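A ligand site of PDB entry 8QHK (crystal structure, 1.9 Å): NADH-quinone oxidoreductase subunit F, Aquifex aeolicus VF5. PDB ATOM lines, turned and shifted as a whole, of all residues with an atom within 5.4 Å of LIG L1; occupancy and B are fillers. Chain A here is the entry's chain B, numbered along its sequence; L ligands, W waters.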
ATOM      1  N   GLY A  65      12.955  23.975  11.970  1.00  0.00           N
ATOM      2  CA  GLY A  65      13.702  25.173  11.624  1.00  0.00           C
ATOM      3  C   GLY A  65      13.450  25.642  10.184  1.00  0.00           C
ATOM      4  O   GLY A  65      13.727  24.927   9.215  1.00  0.00           O
ATOM      5  N   ARG A  66      12.947  26.874  10.085  1.00  0.00           N
ATOM      6  CA  ARG A  66      12.568  27.470   8.822  1.00  0.00           C
ATOM      7  C   ARG A  66      13.754  28.177   8.168  1.00  0.00           C
ATOM      8  O   ARG A  66      13.623  28.736   7.080  1.00  0.00           O
ATOM      9  CB  ARG A  66      11.433  28.479   9.063  1.00  0.00           C
ATOM     10  CG  ARG A  66      10.200  27.895   9.757  1.00  0.00           C
ATOM     11  CD  ARG A  66       9.492  26.866   8.911  1.00  0.00           C
ATOM     12  NE  ARG A  66       8.101  26.715   9.309  1.00  0.00           N
ATOM     13  CZ  ARG A  66       7.543  25.574   9.698  1.00  0.00           C
ATOM     14  NH1 ARG A  66       6.232  25.494   9.835  1.00  0.00           N
ATOM     15  NH2 ARG A  66       8.292  24.513   9.932  1.00  0.00           N
ATOM     16  N   GLY A  67      14.914  28.140   8.836  1.00  0.00           N
ATOM     17  CA  GLY A  67      16.118  28.743   8.290  1.00  0.00           C
ATOM     18  C   GLY A  67      16.717  27.902   7.156  1.00  0.00           C
ATOM     19  O   GLY A  67      17.594  28.400   6.441  1.00  0.00           O
ATOM     20  N   GLY A  68      16.288  26.642   7.042  1.00  0.00           N
ATOM     21  CA  GLY A  68      16.679  25.826   5.898  1.00  0.00           C
ATOM     22  C   GLY A  68      16.968  24.351   6.203  1.00  0.00           C
ATOM     23  O   GLY A  68      16.804  23.522   5.321  1.00  0.00           O
ATOM     24  N   ALA A  69      17.432  24.030   7.427  1.00  0.00           N
ATOM     25  CA  ALA A  69      17.852  22.672   7.757  1.00  0.00           C
ATOM     26  C   ALA A  69      16.735  21.844   8.368  1.00  0.00           C
ATOM     27  O   ALA A  69      16.874  20.627   8.498  1.00  0.00           O
ATOM     28  CB  ALA A  69      19.034  22.698   8.696  1.00  0.00           C
ATOM     29  N   GLY A  70      15.668  22.509   8.841  1.00  0.00           N
ATOM     30  CA  GLY A  70      14.503  21.807   9.369  1.00  0.00           C
ATOM     31  C   GLY A  70      14.752  21.012  10.648  1.00  0.00           C
ATOM     32  O   GLY A  70      14.076  20.016  10.897  1.00  0.00           O
ATOM     33  N   PHE A  71      15.684  21.462  11.502  1.00  0.00           N
ATOM     34  CA  PHE A  71      15.890  20.818  12.789  1.00  0.00           C
ATOM     35  C   PHE A  71      14.680  21.064  13.699  1.00  0.00           C
ATOM     36  O   PHE A  71      14.175  22.174  13.805  1.00  0.00           O
ATOM     37  CB  PHE A  71      17.208  21.265  13.424  1.00  0.00           C
ATOM     38  CG  PHE A  71      17.626  20.428  14.599  1.00  0.00           C
ATOM     39  CD1 PHE A  71      17.143  20.704  15.875  1.00  0.00           C
ATOM     40  CD2 PHE A  71      18.456  19.325  14.439  1.00  0.00           C
ATOM     41  CE1 PHE A  71      17.523  19.927  16.965  1.00  0.00           C
ATOM     42  CE2 PHE A  71      18.821  18.542  15.522  1.00  0.00           C
ATOM     43  CZ  PHE A  71      18.355  18.843  16.785  1.00  0.00           C
ATOM     44  N   THR A  73      12.452  22.223  16.489  1.00  0.00           N
ATOM     45  CA  THR A  73      12.738  23.405  17.274  1.00  0.00           C
ATOM     46  C   THR A  73      12.653  23.082  18.770  1.00  0.00           C
ATOM     47  O   THR A  73      13.557  23.408  19.528  1.00  0.00           O
ATOM     48  CB  THR A  73      11.791  24.541  16.886  1.00  0.00           C
ATOM     49  OG1 THR A  73      11.876  24.691  15.472  1.00  0.00           O
ATOM     50  CG2 THR A  73      12.090  25.841  17.586  1.00  0.00           C
ATOM     51  N   LYS A  76      15.659  21.261  19.886  1.00  0.00           N
ATOM     52  CA  LYS A  76      16.813  22.129  20.053  1.00  0.00           C
ATOM     53  C   LYS A  76      16.764  22.808  21.426  1.00  0.00           C
ATOM     54  O   LYS A  76      17.765  22.846  22.135  1.00  0.00           O
ATOM     55  CB  LYS A  76      16.854  23.178  18.940  1.00  0.00           C
ATOM     56  CG  LYS A  76      18.169  23.967  18.861  1.00  0.00           C
ATOM     57  CD  LYS A  76      18.128  25.149  17.917  1.00  0.00           C
ATOM     58  CE  LYS A  76      17.869  24.745  16.471  1.00  0.00           C
ATOM     59  NZ  LYS A  76      18.120  25.865  15.541  1.00  0.00           N
ATOM     60  N   ASN A  92      18.124  34.743  14.222  1.00  0.00           N
ATOM     61  CA  ASN A  92      18.944  34.847  13.021  1.00  0.00           C
ATOM     62  C   ASN A  92      18.151  35.570  11.941  1.00  0.00           C
ATOM     63  O   ASN A  92      17.255  34.988  11.335  1.00  0.00           O
ATOM     64  CB  ASN A  92      19.379  33.461  12.542  1.00  0.00           C
ATOM     65  CG  ASN A  92      20.439  33.528  11.477  1.00  0.00           C
ATOM     66  OD1 ASN A  92      20.607  34.544  10.798  1.00  0.00           O
ATOM     67  ND2 ASN A  92      21.183  32.444  11.344  1.00  0.00           N
ATOM     68  N   ALA A  93      18.509  36.838  11.682  1.00  0.00           N
ATOM     69  CA  ALA A  93      17.870  37.617  10.633  1.00  0.00           C
ATOM     70  C   ALA A  93      18.903  38.010   9.582  1.00  0.00           C
ATOM     71  O   ALA A  93      18.829  39.102   9.011  1.00  0.00           O
ATOM     72  CB  ALA A  93      17.199  38.836  11.240  1.00  0.00           C
ATOM     73  N   ASP A  94      19.862  37.109   9.294  1.00  0.00           N
ATOM     74  CA  ASP A  94      20.914  37.429   8.352  1.00  0.00           C
ATOM     75  C   ASP A  94      20.484  37.155   6.908  1.00  0.00           C
ATOM     76  O   ASP A  94      21.193  37.557   5.993  1.00  0.00           O
ATOM     77  CB  ASP A  94      22.225  36.707   8.677  1.00  0.00           C
ATOM     78  CG  ASP A  94      23.425  37.367   8.009  1.00  0.00           C
ATOM     79  OD1 ASP A  94      23.679  38.539   8.322  1.00  0.00           O
ATOM     80  OD2 ASP A  94      24.054  36.713   7.144  1.00  0.00           O
ATOM     81  N   GLU A  95      19.330  36.495   6.710  1.00  0.00           N
ATOM     82  CA  GLU A  95      18.772  36.104   5.415  1.00  0.00           C
ATOM     83  C   GLU A  95      19.510  36.698   4.208  1.00  0.00           C
ATOM     84  O   GLU A  95      19.252  37.841   3.816  1.00  0.00           O
ATOM     85  CB  GLU A  95      17.296  36.498   5.369  1.00  0.00           C
ATOM     86  CG  GLU A  95      16.620  36.195   4.035  1.00  0.00           C
ATOM     87  CD  GLU A  95      15.134  36.522   4.052  1.00  0.00           C
ATOM     88  OE1 GLU A  95      14.801  37.733   4.144  1.00  0.00           O
ATOM     89  OE2 GLU A  95      14.326  35.550   4.021  1.00  0.00           O
ATOM     90  N   SER A  96      20.401  35.903   3.607  1.00  0.00           N
ATOM     91  CA  SER A  96      21.235  36.346   2.493  1.00  0.00           C
ATOM     92  C   SER A  96      21.318  35.305   1.379  1.00  0.00           C
ATOM     93  O   SER A  96      22.054  35.527   0.418  1.00  0.00           O
ATOM     94  CB  SER A  96      22.625  36.675   2.992  1.00  0.00           C
ATOM     95  OG  SER A  96      22.612  37.861   3.775  1.00  0.00           O
ATOM     96  N   ASP A 103      11.982  36.337   5.276  1.00  0.00           N
ATOM     97  CA  ASP A 103      12.127  36.794   6.652  1.00  0.00           C
ATOM     98  C   ASP A 103      11.930  38.309   6.746  1.00  0.00           C
ATOM     99  O   ASP A 103      11.380  38.799   7.750  1.00  0.00           O
ATOM    100  CB  ASP A 103      13.488  36.412   7.241  1.00  0.00           C
ATOM    101  CG  ASP A 103      13.726  34.923   7.414  1.00  0.00           C
ATOM    102  OD1 ASP A 103      12.753  34.160   7.334  1.00  0.00           O
ATOM    103  OD2 ASP A 103      14.885  34.527   7.605  1.00  0.00           O
ATOM    104  N   TYR A 180      27.714  36.823   3.985  1.00  0.00           N
ATOM    105  CA  TYR A 180      26.753  35.721   3.945  1.00  0.00           C
ATOM    106  C   TYR A 180      27.021  34.685   5.027  1.00  0.00           C
ATOM    107  O   TYR A 180      26.082  34.079   5.561  1.00  0.00           O
ATOM    108  CB  TYR A 180      26.891  35.046   2.585  1.00  0.00           C
ATOM    109  CG  TYR A 180      26.219  33.710   2.345  1.00  0.00           C
ATOM    110  CD1 TYR A 180      24.849  33.607   2.167  1.00  0.00           C
ATOM    111  CD2 TYR A 180      26.980  32.575   2.169  1.00  0.00           C
ATOM    112  CE1 TYR A 180      24.248  32.391   1.862  1.00  0.00           C
ATOM    113  CE2 TYR A 180      26.400  31.353   1.870  1.00  0.00           C
ATOM    114  CZ  TYR A 180      25.037  31.259   1.711  1.00  0.00           C
ATOM    115  OH  TYR A 180      24.493  30.034   1.385  1.00  0.00           O
ATOM    116  N   ILE A 181      28.311  34.441   5.293  1.00  0.00           N
ATOM    117  CA  ILE A 181      28.729  33.398   6.214  1.00  0.00           C
ATOM    118  C   ILE A 181      28.298  33.709   7.643  1.00  0.00           C
ATOM    119  O   ILE A 181      28.235  32.795   8.464  1.00  0.00           O
ATOM    120  CB  ILE A 181      30.248  33.149   6.119  1.00  0.00           C
ATOM    121  CG1 ILE A 181      30.652  31.852   6.809  1.00  0.00           C
ATOM    122  CG2 ILE A 181      31.053  34.325   6.659  1.00  0.00           C
ATOM    123  CD1 ILE A 181      29.994  30.616   6.250  1.00  0.00           C
ATOM    124  N   GLY A 183      25.450  34.336   8.631  1.00  0.00           N
ATOM    125  CA  GLY A 183      24.190  33.668   8.892  1.00  0.00           C
ATOM    126  C   GLY A 183      24.375  32.241   9.401  1.00  0.00           C
ATOM    127  O   GLY A 183      23.455  31.663   9.982  1.00  0.00           O
ATOM    128  N   GLU A 184      25.555  31.650   9.160  1.00  0.00           N
ATOM    129  CA  GLU A 184      25.886  30.372   9.772  1.00  0.00           C
ATOM    130  C   GLU A 184      25.990  30.598  11.280  1.00  0.00           C
ATOM    131  O   GLU A 184      26.641  31.543  11.708  1.00  0.00           O
ATOM    132  CB  GLU A 184      27.193  29.830   9.160  1.00  0.00           C
ATOM    133  CG  GLU A 184      27.435  28.358   9.434  1.00  0.00           C
ATOM    134  CD  GLU A 184      28.004  28.012  10.801  1.00  0.00           C
ATOM    135  OE1 GLU A 184      28.436  28.923  11.538  1.00  0.00           O
ATOM    136  OE2 GLU A 184      28.012  26.831  11.130  1.00  0.00           O
ATOM    137  N   GLU A 185      25.308  29.778  12.070  1.00  0.00           N
ATOM    138  CA  GLU A 185      24.980  30.137  13.448  1.00  0.00           C
ATOM    139  C   GLU A 185      26.243  30.404  14.278  1.00  0.00           C
ATOM    140  O   GLU A 185      26.201  31.258  15.160  1.00  0.00           O
ATOM    141  CB  GLU A 185      24.109  29.063  14.093  1.00  0.00           C
ATOM    142  CG  GLU A 185      24.744  27.688  14.126  1.00  0.00           C
ATOM    143  CD  GLU A 185      23.890  26.596  14.726  1.00  0.00           C
ATOM    144  OE1 GLU A 185      22.764  26.909  15.182  1.00  0.00           O
ATOM    145  OE2 GLU A 185      24.360  25.442  14.740  1.00  0.00           O
ATOM    146  N   VAL A 218      20.054  29.372  18.571  1.00  0.00           N
ATOM    147  CA  VAL A 218      19.867  30.174  17.382  1.00  0.00           C
ATOM    148  C   VAL A 218      18.647  29.636  16.636  1.00  0.00           C
ATOM    149  O   VAL A 218      18.565  28.433  16.381  1.00  0.00           O
ATOM    150  CB  VAL A 218      21.108  30.182  16.464  1.00  0.00           C
ATOM    151  CG1 VAL A 218      20.917  31.123  15.285  1.00  0.00           C
ATOM    152  CG2 VAL A 218      22.371  30.518  17.233  1.00  0.00           C
ATOM    153  N   ASN A 219      17.710  30.541  16.317  1.00  0.00           N
ATOM    154  CA  ASN A 219      16.549  30.211  15.508  1.00  0.00           C
ATOM    155  C   ASN A 219      16.327  31.298  14.467  1.00  0.00           C
ATOM    156  O   ASN A 219      16.624  32.470  14.669  1.00  0.00           O
ATOM    157  CB  ASN A 219      15.289  29.995  16.359  1.00  0.00           C
ATOM    158  CG  ASN A 219      15.145  28.580  16.872  1.00  0.00           C
ATOM    159  OD1 ASN A 219      14.951  28.366  18.062  1.00  0.00           O
ATOM    160  ND2 ASN A 219      15.209  27.612  15.966  1.00  0.00           N
ATOM    161  N   ASN A 220      15.804  30.864  13.319  1.00  0.00           N
ATOM    162  CA  ASN A 220      15.501  31.729  12.193  1.00  0.00           C
ATOM    163  C   ASN A 220      14.262  32.576  12.515  1.00  0.00           C
ATOM    164  O   ASN A 220      13.392  32.120  13.249  1.00  0.00           O
ATOM    165  CB  ASN A 220      15.282  30.842  10.965  1.00  0.00           C
ATOM    166  CG  ASN A 220      14.714  31.568   9.770  1.00  0.00           C
ATOM    167  OD1 ASN A 220      13.525  31.452   9.495  1.00  0.00           O
ATOM    168  ND2 ASN A 220      15.557  32.309   9.061  1.00  0.00           N
ATOM    169  N   VAL A 221      14.182  33.763  11.915  1.00  0.00           N
ATOM    170  CA  VAL A 221      13.051  34.667  12.033  1.00  0.00           C
ATOM    171  C   VAL A 221      11.720  33.922  11.901  1.00  0.00           C
ATOM    172  O   VAL A 221      10.839  34.035  12.747  1.00  0.00           O
ATOM    173  CB  VAL A 221      13.143  35.798  10.981  1.00  0.00           C
ATOM    174  CG1 VAL A 221      11.844  36.581  10.837  1.00  0.00           C
ATOM    175  CG2 VAL A 221      14.293  36.749  11.260  1.00  0.00           C
ATOM    176  N   THR A 223      10.911  30.734  11.980  1.00  0.00           N
ATOM    177  CA  THR A 223      10.698  29.747  13.035  1.00  0.00           C
ATOM    178  C   THR A 223      10.063  30.437  14.249  1.00  0.00           C
ATOM    179  O   THR A 223       9.033  29.986  14.759  1.00  0.00           O
ATOM    180  CB  THR A 223      11.988  29.061  13.466  1.00  0.00           C
ATOM    181  OG1 THR A 223      12.704  28.643  12.307  1.00  0.00           O
ATOM    182  CG2 THR A 223      11.717  27.907  14.411  1.00  0.00           C
ATOM    183  N   CYS A 393      31.807  23.841   7.997  1.00  0.00           N
ATOM    184  CA  CYS A 393      30.457  24.393   7.935  1.00  0.00           C
ATOM    185  C   CYS A 393      29.794  24.065   6.599  1.00  0.00           C
ATOM    186  O   CYS A 393      30.413  23.547   5.664  1.00  0.00           O
ATOM    187  CB  CYS A 393      30.434  25.906   8.209  1.00  0.00           C
ATOM    188  SG  CYS A 393      30.468  26.976   6.751  1.00  0.00           S
ATOM    189  N   GLY A 394      28.493  24.380   6.539  1.00  0.00           N
ATOM    190  CA  GLY A 394      27.609  23.942   5.471  1.00  0.00           C
ATOM    191  C   GLY A 394      27.899  24.598   4.117  1.00  0.00           C
ATOM    192  O   GLY A 394      27.442  24.098   3.088  1.00  0.00           O
ATOM    193  N   LEU A 395      28.626  25.731   4.112  1.00  0.00           N
ATOM    194  CA  LEU A 395      28.944  26.407   2.865  1.00  0.00           C
ATOM    195  C   LEU A 395      29.863  25.523   2.014  1.00  0.00           C
ATOM    196  O   LEU A 395      29.569  25.265   0.850  1.00  0.00           O
ATOM    197  CB  LEU A 395      29.573  27.772   3.164  1.00  0.00           C
ATOM    198  CG  LEU A 395      29.723  28.694   1.948  1.00  0.00           C
ATOM    199  CD1 LEU A 395      29.742  30.160   2.357  1.00  0.00           C
ATOM    200  CD2 LEU A 395      30.984  28.345   1.150  1.00  0.00           C
HETATM  201  C1  LIG L   1      23.005  29.361   7.450  1.00  0.00           C
HETATM  202  N1  LIG L   1      21.783  29.378   8.200  1.00  0.00           N
HETATM  203  C2  LIG L   1      21.042  30.538   8.220  1.00  0.00           C
HETATM  204  N2  LIG L   1      19.903  30.571   8.984  1.00  0.00           N
HETATM  205  C3  LIG L   1      19.104  31.671   9.087  1.00  0.00           C
HETATM  206  O1  LIG L   1      18.139  31.711   9.848  1.00  0.00           O
HETATM  207  N3  LIG L   1      19.494  32.770   8.354  1.00  0.00           N
HETATM  208  C4  LIG L   1      20.630  32.872   7.558  1.00  0.00           C
HETATM  209  O2  LIG L   1      20.866  33.936   6.978  1.00  0.00           O
HETATM  210  C5  LIG L   1      21.426  31.684   7.538  1.00  0.00           C
HETATM  211  N4  LIG L   1      22.600  31.677   6.858  1.00  0.00           N
HETATM  212  C6  LIG L   1      23.411  30.545   6.815  1.00  0.00           C
HETATM  213  C7  LIG L   1      24.602  30.582   6.090  1.00  0.00           C
HETATM  214  C8  LIG L   1      25.390  29.453   5.980  1.00  0.00           C
HETATM  215  C9  LIG L   1      26.667  29.509   5.167  1.00  0.00           C
HETATM  216  C10 LIG L   1      24.985  28.247   6.605  1.00  0.00           C
HETATM  217  C11 LIG L   1      25.777  26.976   6.433  1.00  0.00           C
HETATM  218  C12 LIG L   1      23.798  28.220   7.338  1.00  0.00           C
HETATM  219  C13 LIG L   1      21.392  28.223   9.026  1.00  0.00           C
HETATM  220  C14 LIG L   1      21.860  28.454  10.472  1.00  0.00           C
HETATM  221  O3  LIG L   1      23.201  27.972  10.586  1.00  0.00           O
HETATM  222  C15 LIG L   1      20.948  27.700  11.449  1.00  0.00           C
HETATM  223  O4  LIG L   1      20.699  26.370  11.004  1.00  0.00           O
HETATM  224  C16 LIG L   1      19.595  28.370  11.714  1.00  0.00           C
HETATM  225  O5  LIG L   1      19.712  29.782  11.951  1.00  0.00           O
HETATM  226  C17 LIG L   1      18.889  27.709  12.875  1.00  0.00           C
HETATM  227  O6  LIG L   1      17.547  28.218  12.985  1.00  0.00           O
HETATM  228  P1  LIG L   1      16.279  27.257  12.617  1.00  0.00           P
HETATM  229  O7  LIG L   1      16.520  25.941  13.328  1.00  0.00           O
HETATM  230  O8  LIG L   1      15.094  28.020  13.194  1.00  0.00           O
HETATM  231  O9  LIG L   1      16.256  27.141  11.113  1.00  0.00           O
HETATM  232  O1  LG2 L   2      19.686  33.119   4.176  1.00  0.00           O
HETATM  233  C1  LG2 L   2      19.349  32.013   4.593  1.00  0.00           C
HETATM  234  C2  LG2 L   2      18.010  31.818   5.225  1.00  0.00           C
HETATM  235  C3  LG2 L   2      20.298  30.885   4.482  1.00  0.00           C
HETATM  236  C4  LG2 L   2      21.652  31.162   3.898  1.00  0.00           C
HETATM  237  C5  LG2 L   2      22.486  29.936   3.809  1.00  0.00           C
HETATM  238  C6  LG2 L   2      22.052  28.745   4.205  1.00  0.00           C
HETATM  239  C7  LG2 L   2      19.956  29.643   4.890  1.00  0.00           C
HETATM  240  N1  LG2 L   2      20.807  28.555   4.757  1.00  0.00           N
HETATM  241  C8  LG2 L   2      20.402  27.219   5.168  1.00  0.00           C
HETATM  242  C9  LG2 L   2      20.378  26.181   4.045  1.00  0.00           C
HETATM  243  O2  LG2 L   2      19.053  25.947   3.553  1.00  0.00           O
HETATM  244  C10 LG2 L   2      20.921  24.900   4.707  1.00  0.00           C
HETATM  245  O3  LG2 L   2      19.937  23.880   4.681  1.00  0.00           O
HETATM  246  O4  LG2 L   2      21.321  26.743   6.130  1.00  0.00           O
HETATM  247  C11 LG2 L   2      21.162  25.310   6.157  1.00  0.00           C
HETATM  248  C12 LG2 L   2      22.360  24.659   6.820  1.00  0.00           C
HETATM  249  O5  LG2 L   2      22.374  25.075   8.202  1.00  0.00           O
HETATM  250  P1  LG2 L   2      23.282  24.368   9.289  1.00  0.00           P
HETATM  251  O6  LG2 L   2      24.624  24.124   8.720  1.00  0.00           O
HETATM  252  O7  LG2 L   2      23.126  25.198  10.509  1.00  0.00           O
HETATM  253  O8  LG2 L   2      22.509  22.967   9.467  1.00  0.00           O
HETATM  254  P2  LG2 L   2      22.585  21.769  10.507  1.00  0.00           P
HETATM  255  O9  LG2 L   2      23.992  21.449  10.842  1.00  0.00           O
HETATM  256  O10 LG2 L   2      21.738  20.682   9.985  1.00  0.00           O
HETATM  257  O11 LG2 L   2      21.917  22.393  11.829  1.00  0.00           O
HETATM  258  C13 LG2 L   2      20.574  22.917  11.847  1.00  0.00           C
HETATM  259  C14 LG2 L   2      20.260  23.408  13.232  1.00  0.00           C
HETATM  260  O12 LG2 L   2      20.060  22.279  14.112  1.00  0.00           O
HETATM  261  C15 LG2 L   2      21.016  22.303  15.167  1.00  0.00           C
HETATM  262  C16 LG2 L   2      22.139  23.245  14.717  1.00  0.00           C
HETATM  263  O13 LG2 L   2      22.822  23.834  15.814  1.00  0.00           O
HETATM  264  C17 LG2 L   2      21.349  24.269  13.901  1.00  0.00           C
HETATM  265  O14 LG2 L   2      20.770  25.223  14.776  1.00  0.00           O
HETATM  266  N2  LG2 L   2      21.459  20.941  15.400  1.00  0.00           N
HETATM  267  C18 LG2 L   2      21.830  20.018  14.454  1.00  0.00           C
HETATM  268  N3  LG2 L   2      22.298  18.898  14.947  1.00  0.00           N
HETATM  269  C19 LG2 L   2      22.247  19.092  16.322  1.00  0.00           C
HETATM  270  C20 LG2 L   2      22.618  18.287  17.414  1.00  0.00           C
HETATM  271  N4  LG2 L   2      23.195  17.089  17.284  1.00  0.00           N
HETATM  272  C21 LG2 L   2      21.730  20.345  16.613  1.00  0.00           C
HETATM  273  N5  LG2 L   2      21.532  20.861  17.832  1.00  0.00           N
HETATM  274  C22 LG2 L   2      21.924  20.008  18.788  1.00  0.00           C
HETATM  275  N6  LG2 L   2      22.436  18.778  18.651  1.00  0.00           N
HETATM  276  O   HOH W   1      23.182  34.509   5.581  1.00  0.00           O
HETATM  277  O   HOH W   2      14.669  24.635  14.860  1.00  0.00           O
HETATM  278  O   HOH W   3      17.391  34.912   8.546  1.00  0.00           O
HETATM  279  O   HOH W   4      17.120  23.912  11.628  1.00  0.00           O
HETATM  280  O   HOH W   5      18.164  25.794   9.753  1.00  0.00           O
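The side-chain hydroxyl of Thr 223 sits at hydrogen-bond distance from an oxygen (O8) of LIG L1, 2.6 Å away.
NZ of Lys 76 is in salt-bridge range of O7 of LIG L1 (2.7 Å).
The backbone NH of Asn 220 is in hydrogen-bond range of an oxygen (O8) of LIG L1.
An oxygen (O1) of LIG L1 sits at hydrogen-bond distance from the side-chain amide nitrogen (ND2) of Asn 220 (2.8 Å).
The side-chain amide nitrogen (ND2) of Asn 219 is in hydrogen-bond range of an oxygen (O8) of LIG L1 (2.8 Å).
N of Gly 67 is in hydrogen-bond range of O9 of LIG L1.
The backbone NH (N) of Glu 95 sits at hydrogen-bond distance from an oxygen (O2) of LIG L1 (3.0 Å).
ND2 of Asn 92 lies within hydrogen-bond range of O5 of LIG L1 (3.1 Å).
An oxygen (O3) of LIG L1 sits at hydrogen-bond distance from the backbone NH (N) of Glu 185 (3.1 Å).
O of Gly 183 sits close to N4 of LIG L1 (3.2 Å).
The backbone NH (N) of Arg 66 sits at hydrogen-bond distance from an oxygen (O9) of LIG L1.
O14 of LG2 L2 sits at hydrogen-bond distance from NZ of Lys 76 (2.8 Å).
OE2 of Glu 185 sits at hydrogen-bond distance from O13 of LG2 L2, 2.5 Å away.
An oxygen (O1) of LG2 L2 lies within hydrogen-bond range of the backbone NH (N) of Ser 96, at 2.9 Å.
The backbone carbonyl oxygen of Gly 68 is in hydrogen-bond range of an oxygen (O3) of LG2 L2 (3.2 Å).
Merely in contact with LIG L1: Asp 94 (3.2 Å), Gly 65 (3.3 Å), Glu 184 (3.4 Å), Val 218 (3.6 Å), Ile 181 (3.7 Å), Gly 394 (3.7 Å), Tyr 180 (3.8 Å), Leu 395 (3.9 Å) and Ser 96 (3.9 Å).
Hydrophobic or aromatic side chains that line LIG L1: Tyr 180, Ile 181, Val 218 and Leu 395.
19 residues have an atom within 4 Å of LIG L1: Gly 65, Arg 66, Gly 67, Lys 76, Asn 92, Asp 94, Glu 95, Ser 96, Tyr 180, Ile 181, Gly 183, Glu 184, Glu 185, Val 218, Asn 219, Asn 220, Thr 223, Gly 394 and Leu 395.
N of Arg 66 lies within hydrogen-bond range of OG1 of Thr 223 (2.9 Å).
The side-chain amide nitrogen (ND2) of Asn 219 sits close to the side-chain amino group (NZ) of Lys 76, at 3.4 Å.
The backbone NH (N) of Asn 92 lies within hydrogen-bond range of the backbone carbonyl oxygen (O) of Asn 219 (2.8 Å).
ND2 of Asn 92 lies within hydrogen-bond range of O of Gly 183 (2.8 Å).
N of Asp 94 sits at hydrogen-bond distance from OD1 of Asn 92, at 3.1 Å.
OG of Ser 96 sits at hydrogen-bond distance from O of Asp 94, at 2.7 Å.
O of Phe 71 is in hydrogen-bond range of N of Gly 65, 2.8 Å away.
The backbone carbonyl oxygen (O) of Gly 65 sits at hydrogen-bond distance from the backbone NH (N) of Gly 70 (3.1 Å).
Water W5 lies within hydrogen-bond range of an oxygen (O9) of LIG L1 (2.7 Å), the backbone NH of Ala 69 (3.0 Å) and the backbone NH of Gly 68 (3.4 Å).
Water W4 lies within hydrogen-bond range of an oxygen (O7) of LIG L1 (2.7 Å), the backbone NH (N) of Phe 71 (2.8 Å) and the backbone NH (N) of Gly 70 (3.4 Å).
Water W2 lies within hydrogen-bond range of the backbone carbonyl oxygen (O) of Phe 71 (2.7 Å), an oxygen (O7) of LIG L1 (2.7 Å), the side-chain hydroxyl (OG1) of Thr 73 (2.9 Å), the side-chain amide nitrogen (ND2) of Asn 219 (3.2 Å) and the backbone NH (N) of Gly 65 (3.4 Å).
O7 of LG2 L2 sits at hydrogen-bond distance from O4 of LIG L1.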
